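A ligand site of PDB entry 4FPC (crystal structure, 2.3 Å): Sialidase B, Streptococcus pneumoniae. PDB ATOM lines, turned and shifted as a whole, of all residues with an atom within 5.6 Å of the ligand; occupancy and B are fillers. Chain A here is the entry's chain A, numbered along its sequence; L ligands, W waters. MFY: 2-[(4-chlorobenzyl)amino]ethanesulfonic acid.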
ATOM      1  N   ARG A 245      22.133  35.867  -7.427  1.00  0.00           N
ATOM      2  CA  ARG A 245      22.356  34.461  -7.749  1.00  0.00           C
ATOM      3  C   ARG A 245      21.071  33.751  -8.148  1.00  0.00           C
ATOM      4  O   ARG A 245      19.967  34.231  -7.884  1.00  0.00           O
ATOM      5  CB  ARG A 245      23.032  33.692  -6.578  1.00  0.00           C
ATOM      6  CG  ARG A 245      24.543  33.908  -6.503  1.00  0.00           C
ATOM      7  CD  ARG A 245      25.282  32.734  -5.847  1.00  0.00           C
ATOM      8  NE  ARG A 245      25.045  31.481  -6.561  1.00  0.00           N
ATOM      9  CZ  ARG A 245      25.437  30.281  -6.139  1.00  0.00           C
ATOM     10  NH1 ARG A 245      26.110  30.131  -4.986  1.00  0.00           N
ATOM     11  NH2 ARG A 245      25.166  29.222  -6.887  1.00  0.00           N
ATOM     12  N   ILE A 246      21.224  32.593  -8.782  1.00  0.00           N
ATOM     13  CA  ILE A 246      20.123  31.667  -8.995  1.00  0.00           C
ATOM     14  C   ILE A 246      19.107  32.273  -9.991  1.00  0.00           C
ATOM     15  O   ILE A 246      17.966  32.578  -9.630  1.00  0.00           O
ATOM     16  CB  ILE A 246      19.431  31.265  -7.649  1.00  0.00           C
ATOM     17  CG1 ILE A 246      20.429  31.141  -6.481  1.00  0.00           C
ATOM     18  CG2 ILE A 246      18.667  29.978  -7.797  1.00  0.00           C
ATOM     19  CD1 ILE A 246      21.601  30.193  -6.738  1.00  0.00           C
ATOM     20  N   ARG A 264      20.563  39.119  -3.643  1.00  0.00           N
ATOM     21  CA  ARG A 264      21.355  38.837  -2.439  1.00  0.00           C
ATOM     22  C   ARG A 264      22.088  40.056  -1.873  1.00  0.00           C
ATOM     23  O   ARG A 264      22.968  40.632  -2.523  1.00  0.00           O
ATOM     24  CB  ARG A 264      22.305  37.667  -2.676  1.00  0.00           C
ATOM     25  CG  ARG A 264      21.595  36.403  -3.148  1.00  0.00           C
ATOM     26  CD  ARG A 264      22.462  35.186  -2.991  1.00  0.00           C
ATOM     27  NE  ARG A 264      21.731  33.965  -3.249  1.00  0.00           N
ATOM     28  CZ  ARG A 264      22.261  32.750  -3.176  1.00  0.00           C
ATOM     29  NH1 ARG A 264      23.545  32.593  -2.843  1.00  0.00           N
ATOM     30  NH2 ARG A 264      21.508  31.692  -3.436  1.00  0.00           N
ATOM     31  N   ASP A 270      24.618  32.024   0.360  1.00  0.00           N
ATOM     32  CA  ASP A 270      23.329  31.350   0.567  1.00  0.00           C
ATOM     33  C   ASP A 270      22.749  31.818   1.902  1.00  0.00           C
ATOM     34  O   ASP A 270      23.475  32.347   2.758  1.00  0.00           O
ATOM     35  CB  ASP A 270      23.519  29.830   0.720  1.00  0.00           C
ATOM     36  CG  ASP A 270      23.729  29.099  -0.606  1.00  0.00           C
ATOM     37  OD1 ASP A 270      24.141  27.919  -0.540  1.00  0.00           O
ATOM     38  OD2 ASP A 270      23.503  29.675  -1.680  1.00  0.00           O
ATOM     39  N   SER A 271      21.457  31.589   2.097  1.00  0.00           N
ATOM     40  CA  SER A 271      20.854  31.678   3.424  1.00  0.00           C
ATOM     41  C   SER A 271      21.640  30.793   4.425  1.00  0.00           C
ATOM     42  O   SER A 271      22.059  29.700   4.064  1.00  0.00           O
ATOM     43  CB  SER A 271      19.394  31.244   3.379  1.00  0.00           C
ATOM     44  OG  SER A 271      18.656  32.107   2.548  1.00  0.00           O
ATOM     45  N   ILE A 326      15.044  32.109  -1.120  1.00  0.00           N
ATOM     46  CA  ILE A 326      16.148  31.552  -1.912  1.00  0.00           C
ATOM     47  C   ILE A 326      15.613  30.484  -2.858  1.00  0.00           C
ATOM     48  O   ILE A 326      14.652  29.781  -2.524  1.00  0.00           O
ATOM     49  CB  ILE A 326      17.317  31.004  -0.983  1.00  0.00           C
ATOM     50  CG1 ILE A 326      18.429  30.353  -1.789  1.00  0.00           C
ATOM     51  CG2 ILE A 326      16.804  30.020   0.078  1.00  0.00           C
ATOM     52  CD1 ILE A 326      19.655  29.992  -0.939  1.00  0.00           C
ATOM     53  N   ASP A 327      16.224  30.375  -4.036  1.00  0.00           N
ATOM     54  CA  ASP A 327      15.880  29.339  -5.029  1.00  0.00           C
ATOM     55  C   ASP A 327      14.450  29.424  -5.591  1.00  0.00           C
ATOM     56  O   ASP A 327      13.593  28.624  -5.230  1.00  0.00           O
ATOM     57  CB  ASP A 327      16.113  27.930  -4.475  1.00  0.00           C
ATOM     58  CG  ASP A 327      17.582  27.601  -4.306  1.00  0.00           C
ATOM     59  OD1 ASP A 327      18.451  28.374  -4.772  1.00  0.00           O
ATOM     60  OD2 ASP A 327      17.865  26.556  -3.685  1.00  0.00           O
ATOM     61  N   ASP A 344      12.008  28.988  -1.752  1.00  0.00           N
ATOM     62  CA  ASP A 344      12.185  28.634  -0.342  1.00  0.00           C
ATOM     63  C   ASP A 344      12.061  29.876   0.550  1.00  0.00           C
ATOM     64  O   ASP A 344      12.484  30.974   0.173  1.00  0.00           O
ATOM     65  CB  ASP A 344      13.551  27.980  -0.079  1.00  0.00           C
ATOM     66  CG  ASP A 344      13.772  26.724  -0.888  1.00  0.00           C
ATOM     67  OD1 ASP A 344      12.792  26.011  -1.183  1.00  0.00           O
ATOM     68  OD2 ASP A 344      14.946  26.433  -1.226  1.00  0.00           O
ATOM     69  N   MET A 346      12.966  31.246   4.459  1.00  0.00           N
ATOM     70  CA  MET A 346      13.751  31.033   5.690  1.00  0.00           C
ATOM     71  C   MET A 346      13.407  32.075   6.740  1.00  0.00           C
ATOM     72  O   MET A 346      13.531  33.275   6.486  1.00  0.00           O
ATOM     73  CB  MET A 346      15.255  31.151   5.401  1.00  0.00           C
ATOM     74  CG  MET A 346      15.766  30.222   4.327  1.00  0.00           C
ATOM     75  SD  MET A 346      15.531  28.485   4.745  1.00  0.00           S
ATOM     76  CE  MET A 346      14.557  27.970   3.345  1.00  0.00           C
ATOM     77  N   ILE A 350      18.029  31.413   9.490  1.00  0.00           N
ATOM     78  CA  ILE A 350      18.018  30.008   9.066  1.00  0.00           C
ATOM     79  C   ILE A 350      18.500  29.837   7.627  1.00  0.00           C
ATOM     80  O   ILE A 350      18.213  30.657   6.764  1.00  0.00           O
ATOM     81  CB  ILE A 350      16.620  29.383   9.216  1.00  0.00           C
ATOM     82  CG1 ILE A 350      16.094  29.596  10.636  1.00  0.00           C
ATOM     83  CG2 ILE A 350      16.646  27.902   8.810  1.00  0.00           C
ATOM     84  CD1 ILE A 350      17.056  29.134  11.721  1.00  0.00           C
ATOM     85  N   GLY A 351      19.266  28.763   7.407  1.00  0.00           N
ATOM     86  CA  GLY A 351      19.679  28.305   6.087  1.00  0.00           C
ATOM     87  C   GLY A 351      19.585  26.794   6.097  1.00  0.00           C
ATOM     88  O   GLY A 351      19.024  26.219   7.029  1.00  0.00           O
ATOM     89  N   ASN A 352      20.146  26.118   5.092  1.00  0.00           N
ATOM     90  CA  ASN A 352      19.932  24.672   4.983  1.00  0.00           C
ATOM     91  C   ASN A 352      20.735  23.812   5.982  1.00  0.00           C
ATOM     92  O   ASN A 352      20.526  22.600   6.086  1.00  0.00           O
ATOM     93  CB  ASN A 352      20.117  24.172   3.536  1.00  0.00           C
ATOM     94  CG  ASN A 352      21.565  24.243   3.068  1.00  0.00           C
ATOM     95  OD1 ASN A 352      22.363  25.004   3.599  1.00  0.00           O
ATOM     96  ND2 ASN A 352      21.887  23.453   2.049  1.00  0.00           N
ATOM     97  N   ASN A 457      13.025  25.112   7.149  1.00  0.00           N
ATOM     98  CA  ASN A 457      12.859  25.534   5.762  1.00  0.00           C
ATOM     99  C   ASN A 457      11.419  25.322   5.258  1.00  0.00           C
ATOM    100  O   ASN A 457      10.834  24.250   5.413  1.00  0.00           O
ATOM    101  CB  ASN A 457      13.869  24.813   4.848  1.00  0.00           C
ATOM    102  CG  ASN A 457      13.792  23.287   4.983  1.00  0.00           C
ATOM    103  OD1 ASN A 457      13.867  22.749   6.093  1.00  0.00           O
ATOM    104  ND2 ASN A 457      13.644  22.593   3.852  1.00  0.00           N
ATOM    105  N   TYR A 489      13.451  21.073  -0.500  1.00  0.00           N
ATOM    106  CA  TYR A 489      14.023  22.284  -1.071  1.00  0.00           C
ATOM    107  C   TYR A 489      13.667  22.404  -2.554  1.00  0.00           C
ATOM    108  O   TYR A 489      13.838  21.458  -3.324  1.00  0.00           O
ATOM    109  CB  TYR A 489      15.541  22.291  -0.908  1.00  0.00           C
ATOM    110  CG  TYR A 489      15.991  22.433   0.530  1.00  0.00           C
ATOM    111  CD1 TYR A 489      16.100  23.682   1.115  1.00  0.00           C
ATOM    112  CD2 TYR A 489      16.305  21.315   1.301  1.00  0.00           C
ATOM    113  CE1 TYR A 489      16.507  23.820   2.410  1.00  0.00           C
ATOM    114  CE2 TYR A 489      16.719  21.448   2.601  1.00  0.00           C
ATOM    115  CZ  TYR A 489      16.823  22.698   3.158  1.00  0.00           C
ATOM    116  OH  TYR A 489      17.249  22.872   4.458  1.00  0.00           O
ATOM    117  N   TYR A 509      13.845  18.805  -3.752  1.00  0.00           N
ATOM    118  CA  TYR A 509      14.688  17.717  -3.275  1.00  0.00           C
ATOM    119  C   TYR A 509      14.805  17.697  -1.758  1.00  0.00           C
ATOM    120  O   TYR A 509      14.642  18.705  -1.072  1.00  0.00           O
ATOM    121  CB  TYR A 509      16.085  17.800  -3.899  1.00  0.00           C
ATOM    122  CG  TYR A 509      16.897  19.013  -3.483  1.00  0.00           C
ATOM    123  CD1 TYR A 509      17.671  19.000  -2.326  1.00  0.00           C
ATOM    124  CD2 TYR A 509      16.877  20.166  -4.246  1.00  0.00           C
ATOM    125  CE1 TYR A 509      18.401  20.108  -1.930  1.00  0.00           C
ATOM    126  CE2 TYR A 509      17.617  21.292  -3.865  1.00  0.00           C
ATOM    127  CZ  TYR A 509      18.368  21.246  -2.706  1.00  0.00           C
ATOM    128  OH  TYR A 509      19.095  22.343  -2.332  1.00  0.00           O
ATOM    129  N   THR A 539      22.476  17.872  -3.048  1.00  0.00           N
ATOM    130  CA  THR A 539      21.780  19.052  -3.525  1.00  0.00           C
ATOM    131  C   THR A 539      21.284  18.663  -4.910  1.00  0.00           C
ATOM    132  O   THR A 539      21.918  18.983  -5.919  1.00  0.00           O
ATOM    133  CB  THR A 539      22.727  20.265  -3.601  1.00  0.00           C
ATOM    134  OG1 THR A 539      23.386  20.454  -2.341  1.00  0.00           O
ATOM    135  CG2 THR A 539      21.941  21.544  -3.963  1.00  0.00           C
ATOM    136  N   GLU A 541      19.486  19.341  -7.512  1.00  0.00           N
ATOM    137  CA  GLU A 541      18.746  20.347  -8.263  1.00  0.00           C
ATOM    138  C   GLU A 541      18.331  19.767  -9.615  1.00  0.00           C
ATOM    139  O   GLU A 541      19.158  19.418 -10.455  1.00  0.00           O
ATOM    140  CB  GLU A 541      19.580  21.624  -8.416  1.00  0.00           C
ATOM    141  CG  GLU A 541      19.677  22.392  -7.113  1.00  0.00           C
ATOM    142  CD  GLU A 541      20.940  23.222  -6.977  1.00  0.00           C
ATOM    143  OE1 GLU A 541      20.940  24.171  -6.165  1.00  0.00           O
ATOM    144  OE2 GLU A 541      21.935  22.936  -7.671  1.00  0.00           O
ATOM    145  N   ARG A 557      21.428  17.376 -10.647  1.00  0.00           N
ATOM    146  CA  ARG A 557      22.793  17.492 -10.164  1.00  0.00           C
ATOM    147  C   ARG A 557      23.020  16.380  -9.162  1.00  0.00           C
ATOM    148  O   ARG A 557      22.129  16.067  -8.381  1.00  0.00           O
ATOM    149  CB  ARG A 557      22.959  18.889  -9.531  1.00  0.00           C
ATOM    150  CG  ARG A 557      24.103  19.090  -8.543  1.00  0.00           C
ATOM    151  CD  ARG A 557      23.968  20.461  -7.851  1.00  0.00           C
ATOM    152  NE  ARG A 557      25.045  20.709  -6.886  1.00  0.00           N
ATOM    153  CZ  ARG A 557      25.234  21.868  -6.240  1.00  0.00           C
ATOM    154  NH1 ARG A 557      24.411  22.902  -6.436  1.00  0.00           N
ATOM    155  NH2 ARG A 557      26.239  21.988  -5.376  1.00  0.00           N
ATOM    156  N   GLY A 590      29.005  19.289  -7.927  1.00  0.00           N
ATOM    157  CA  GLY A 590      27.999  19.580  -8.920  1.00  0.00           C
ATOM    158  C   GLY A 590      27.567  21.029  -9.048  1.00  0.00           C
ATOM    159  O   GLY A 590      28.007  21.926  -8.331  1.00  0.00           O
ATOM    160  N   ARG A 619      33.574  25.390 -11.595  1.00  0.00           N
ATOM    161  CA  ARG A 619      32.372  25.830 -12.308  1.00  0.00           C
ATOM    162  C   ARG A 619      32.813  26.764 -13.409  1.00  0.00           C
ATOM    163  O   ARG A 619      32.818  27.970 -13.239  1.00  0.00           O
ATOM    164  CB  ARG A 619      31.366  26.501 -11.369  1.00  0.00           C
ATOM    165  CG  ARG A 619      30.761  25.518 -10.371  1.00  0.00           C
ATOM    166  CD  ARG A 619      29.790  26.178  -9.396  1.00  0.00           C
ATOM    167  NE  ARG A 619      28.933  25.177  -8.757  1.00  0.00           N
ATOM    168  CZ  ARG A 619      28.093  25.449  -7.753  1.00  0.00           C
ATOM    169  NH1 ARG A 619      28.019  26.685  -7.273  1.00  0.00           N
ATOM    170  NH2 ARG A 619      27.351  24.479  -7.226  1.00  0.00           N
ATOM    171  N   TYR A 653      25.402  28.393 -12.063  1.00  0.00           N
ATOM    172  CA  TYR A 653      23.967  28.180 -12.208  1.00  0.00           C
ATOM    173  C   TYR A 653      23.499  28.892 -13.462  1.00  0.00           C
ATOM    174  O   TYR A 653      24.072  29.918 -13.848  1.00  0.00           O
ATOM    175  CB  TYR A 653      23.195  28.727 -11.001  1.00  0.00           C
ATOM    176  CG  TYR A 653      23.140  27.822  -9.780  1.00  0.00           C
ATOM    177  CD1 TYR A 653      24.285  27.182  -9.311  1.00  0.00           C
ATOM    178  CD2 TYR A 653      21.961  27.636  -9.077  1.00  0.00           C
ATOM    179  CE1 TYR A 653      24.258  26.359  -8.199  1.00  0.00           C
ATOM    180  CE2 TYR A 653      21.913  26.818  -7.954  1.00  0.00           C
ATOM    181  CZ  TYR A 653      23.064  26.195  -7.514  1.00  0.00           C
ATOM    182  OH  TYR A 653      23.048  25.377  -6.411  1.00  0.00           O
ATOM    183  N   SER A 673      30.759  30.073  -8.724  1.00  0.00           N
ATOM    184  CA  SER A 673      29.985  30.459  -7.553  1.00  0.00           C
ATOM    185  C   SER A 673      30.193  29.470  -6.398  1.00  0.00           C
ATOM    186  O   SER A 673      29.533  29.566  -5.363  1.00  0.00           O
ATOM    187  CB  SER A 673      28.509  30.641  -7.915  1.00  0.00           C
ATOM    188  OG  SER A 673      27.937  29.414  -8.367  1.00  0.00           O
ATOM    189  N   TRP A 674      31.125  28.539  -6.582  1.00  0.00           N
ATOM    190  CA  TRP A 674      31.524  27.642  -5.513  1.00  0.00           C
ATOM    191  C   TRP A 674      32.824  28.148  -4.890  1.00  0.00           C
ATOM    192  O   TRP A 674      32.982  28.175  -3.666  1.00  0.00           O
ATOM    193  CB  TRP A 674      31.677  26.209  -6.032  1.00  0.00           C
ATOM    194  CG  TRP A 674      31.890  25.163  -4.945  1.00  0.00           C
ATOM    195  CD1 TRP A 674      33.082  24.674  -4.484  1.00  0.00           C
ATOM    196  CD2 TRP A 674      30.872  24.470  -4.205  1.00  0.00           C
ATOM    197  NE1 TRP A 674      32.871  23.726  -3.511  1.00  0.00           N
ATOM    198  CE2 TRP A 674      31.521  23.589  -3.315  1.00  0.00           C
ATOM    199  CE3 TRP A 674      29.467  24.518  -4.198  1.00  0.00           C
ATOM    200  CZ2 TRP A 674      30.815  22.756  -2.429  1.00  0.00           C
ATOM    201  CZ3 TRP A 674      28.771  23.690  -3.320  1.00  0.00           C
ATOM    202  CH2 TRP A 674      29.440  22.818  -2.448  1.00  0.00           C
HETATM  203  CAG MFY L   1      21.164  26.562   0.693  1.00  0.00           C
HETATM  204  CAE MFY L   1      20.384  27.081   1.628  1.00  0.00           C
HETATM  205  CAM MFY L   1      18.970  27.073   1.460  1.00  0.00           C
HETATM  206 CL   MFY L   1      17.998  27.741   2.688  1.00  0.00          CL
HETATM  207  CAF MFY L   1      18.406  26.542   0.324  1.00  0.00           C
HETATM  208  CAH MFY L   1      19.240  26.004  -0.671  1.00  0.00           C
HETATM  209  CAN MFY L   1      20.592  26.008  -0.486  1.00  0.00           C
HETATM  210  CAK MFY L   1      21.520  25.425  -1.507  1.00  0.00           C
HETATM  211  NAL MFY L   1      22.284  26.417  -2.339  1.00  0.00           N
HETATM  212  CAI MFY L   1      23.390  25.731  -3.009  1.00  0.00           C
HETATM  213  CAJ MFY L   1      24.202  26.626  -3.868  1.00  0.00           C
HETATM  214  SAO MFY L   1      25.903  26.221  -4.140  1.00  0.00           S
HETATM  215  OAC MFY L   1      26.466  27.253  -5.048  1.00  0.00           O
HETATM  216  OAB MFY L   1      26.014  24.848  -4.770  1.00  0.00           O
HETATM  217  OAA MFY L   1      26.600  26.234  -2.889  1.00  0.00           O
HETATM  218  O   HOH W   1      19.557  24.509  -4.062  1.00  0.00           O
HETATM  219  O   HOH W   2      19.193  22.829   0.315  1.00  0.00           O
HETATM  220  O   HOH W   3      21.264  27.966  -3.968  1.00  0.00           O
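Water W3 bridges a nitrogen (NAL) of the ligand (2.5 Å) and the side-chain carboxylate of Asp 327 (3.0 Å). Water W2 bridges the side-chain hydroxyl of Tyr 509 and the side-chain amide nitrogen of Asn 352. Water W1 lies within hydrogen-bond range of the side-chain carboxylate of Glu 541 (2.5 Å), the side-chain carboxylate of Asp 327 (2.7 Å) and the side-chain hydroxyl of Tyr 509 (2.8 Å).
The guanidinium group (NH1) of Arg 619 is in salt-bridge range of an oxygen (OAC) of the ligand, 2.8 Å away. NH1 of Arg 245 is in salt-bridge range of OAC of the ligand. NH2 of Arg 557 lies within salt-bridge range of OAB of the ligand (2.9 Å). The side-chain carboxylate of Asp 270 is in salt-bridge range of a nitrogen (NAL) of the ligand (3.0 Å). OH of Tyr 653 sits close to OAB of the ligand (3.4 Å).
CB of Ser 271 touches CL of the ligand, at 3.8 Å. Ile 326 touches the ligand (CG2 to CL, 3.7 Å). OD2 of Asp 327 touches CAH of the ligand, at 3.4 Å. Asp 344 touches the ligand. Met 346 touches the ligand. CA of Gly 351 touches CL of the ligand (3.8 Å). Asn 352 touches the ligand (CG to CAG, 3.3 Å). Tyr 489 touches the ligand. O of Ser 673 touches OAC of the ligand, 3.9 Å away. CZ3 of Trp 674 touches OAB of the ligand, 3.3 Å away. Hydrophobic or aromatic side chains that line the ligand: Ile 326, Met 346, Tyr 489, Tyr 653 and Trp 674. Of the 23 residues printed, 15 come within 4 Å of the ligand.
The guanidinium group of Arg 619 sits at hydrogen-bond distance from the side-chain hydroxyl of Ser 673 (2.9 Å). O of Gly 590 is in hydrogen-bond range of NH2 of Arg 619, 2.9 Å away. The guanidinium group (NH2) of Arg 245 sits at hydrogen-bond distance from the side-chain hydroxyl (OG) of Ser 673, 3.1 Å away. NH1 of Arg 557 lies within hydrogen-bond range of OH of Tyr 653, 2.8 Å away. The guanidinium group (NH1) of Arg 557 lies within salt-bridge range of the side-chain carboxylate (OE2) of Glu 541 (2.8 Å). The backbone carbonyl oxygen of Gly 590 lies within hydrogen-bond range of the guanidinium group of Arg 557 (3.4 Å). The side-chain hydroxyl (OH) of Tyr 653 sits at hydrogen-bond distance from the side-chain carboxylate (OE1) of Glu 541, 2.4 Å away. O of Ile 326 is in hydrogen-bond range of N of Asp 344, 2.9 Å away.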
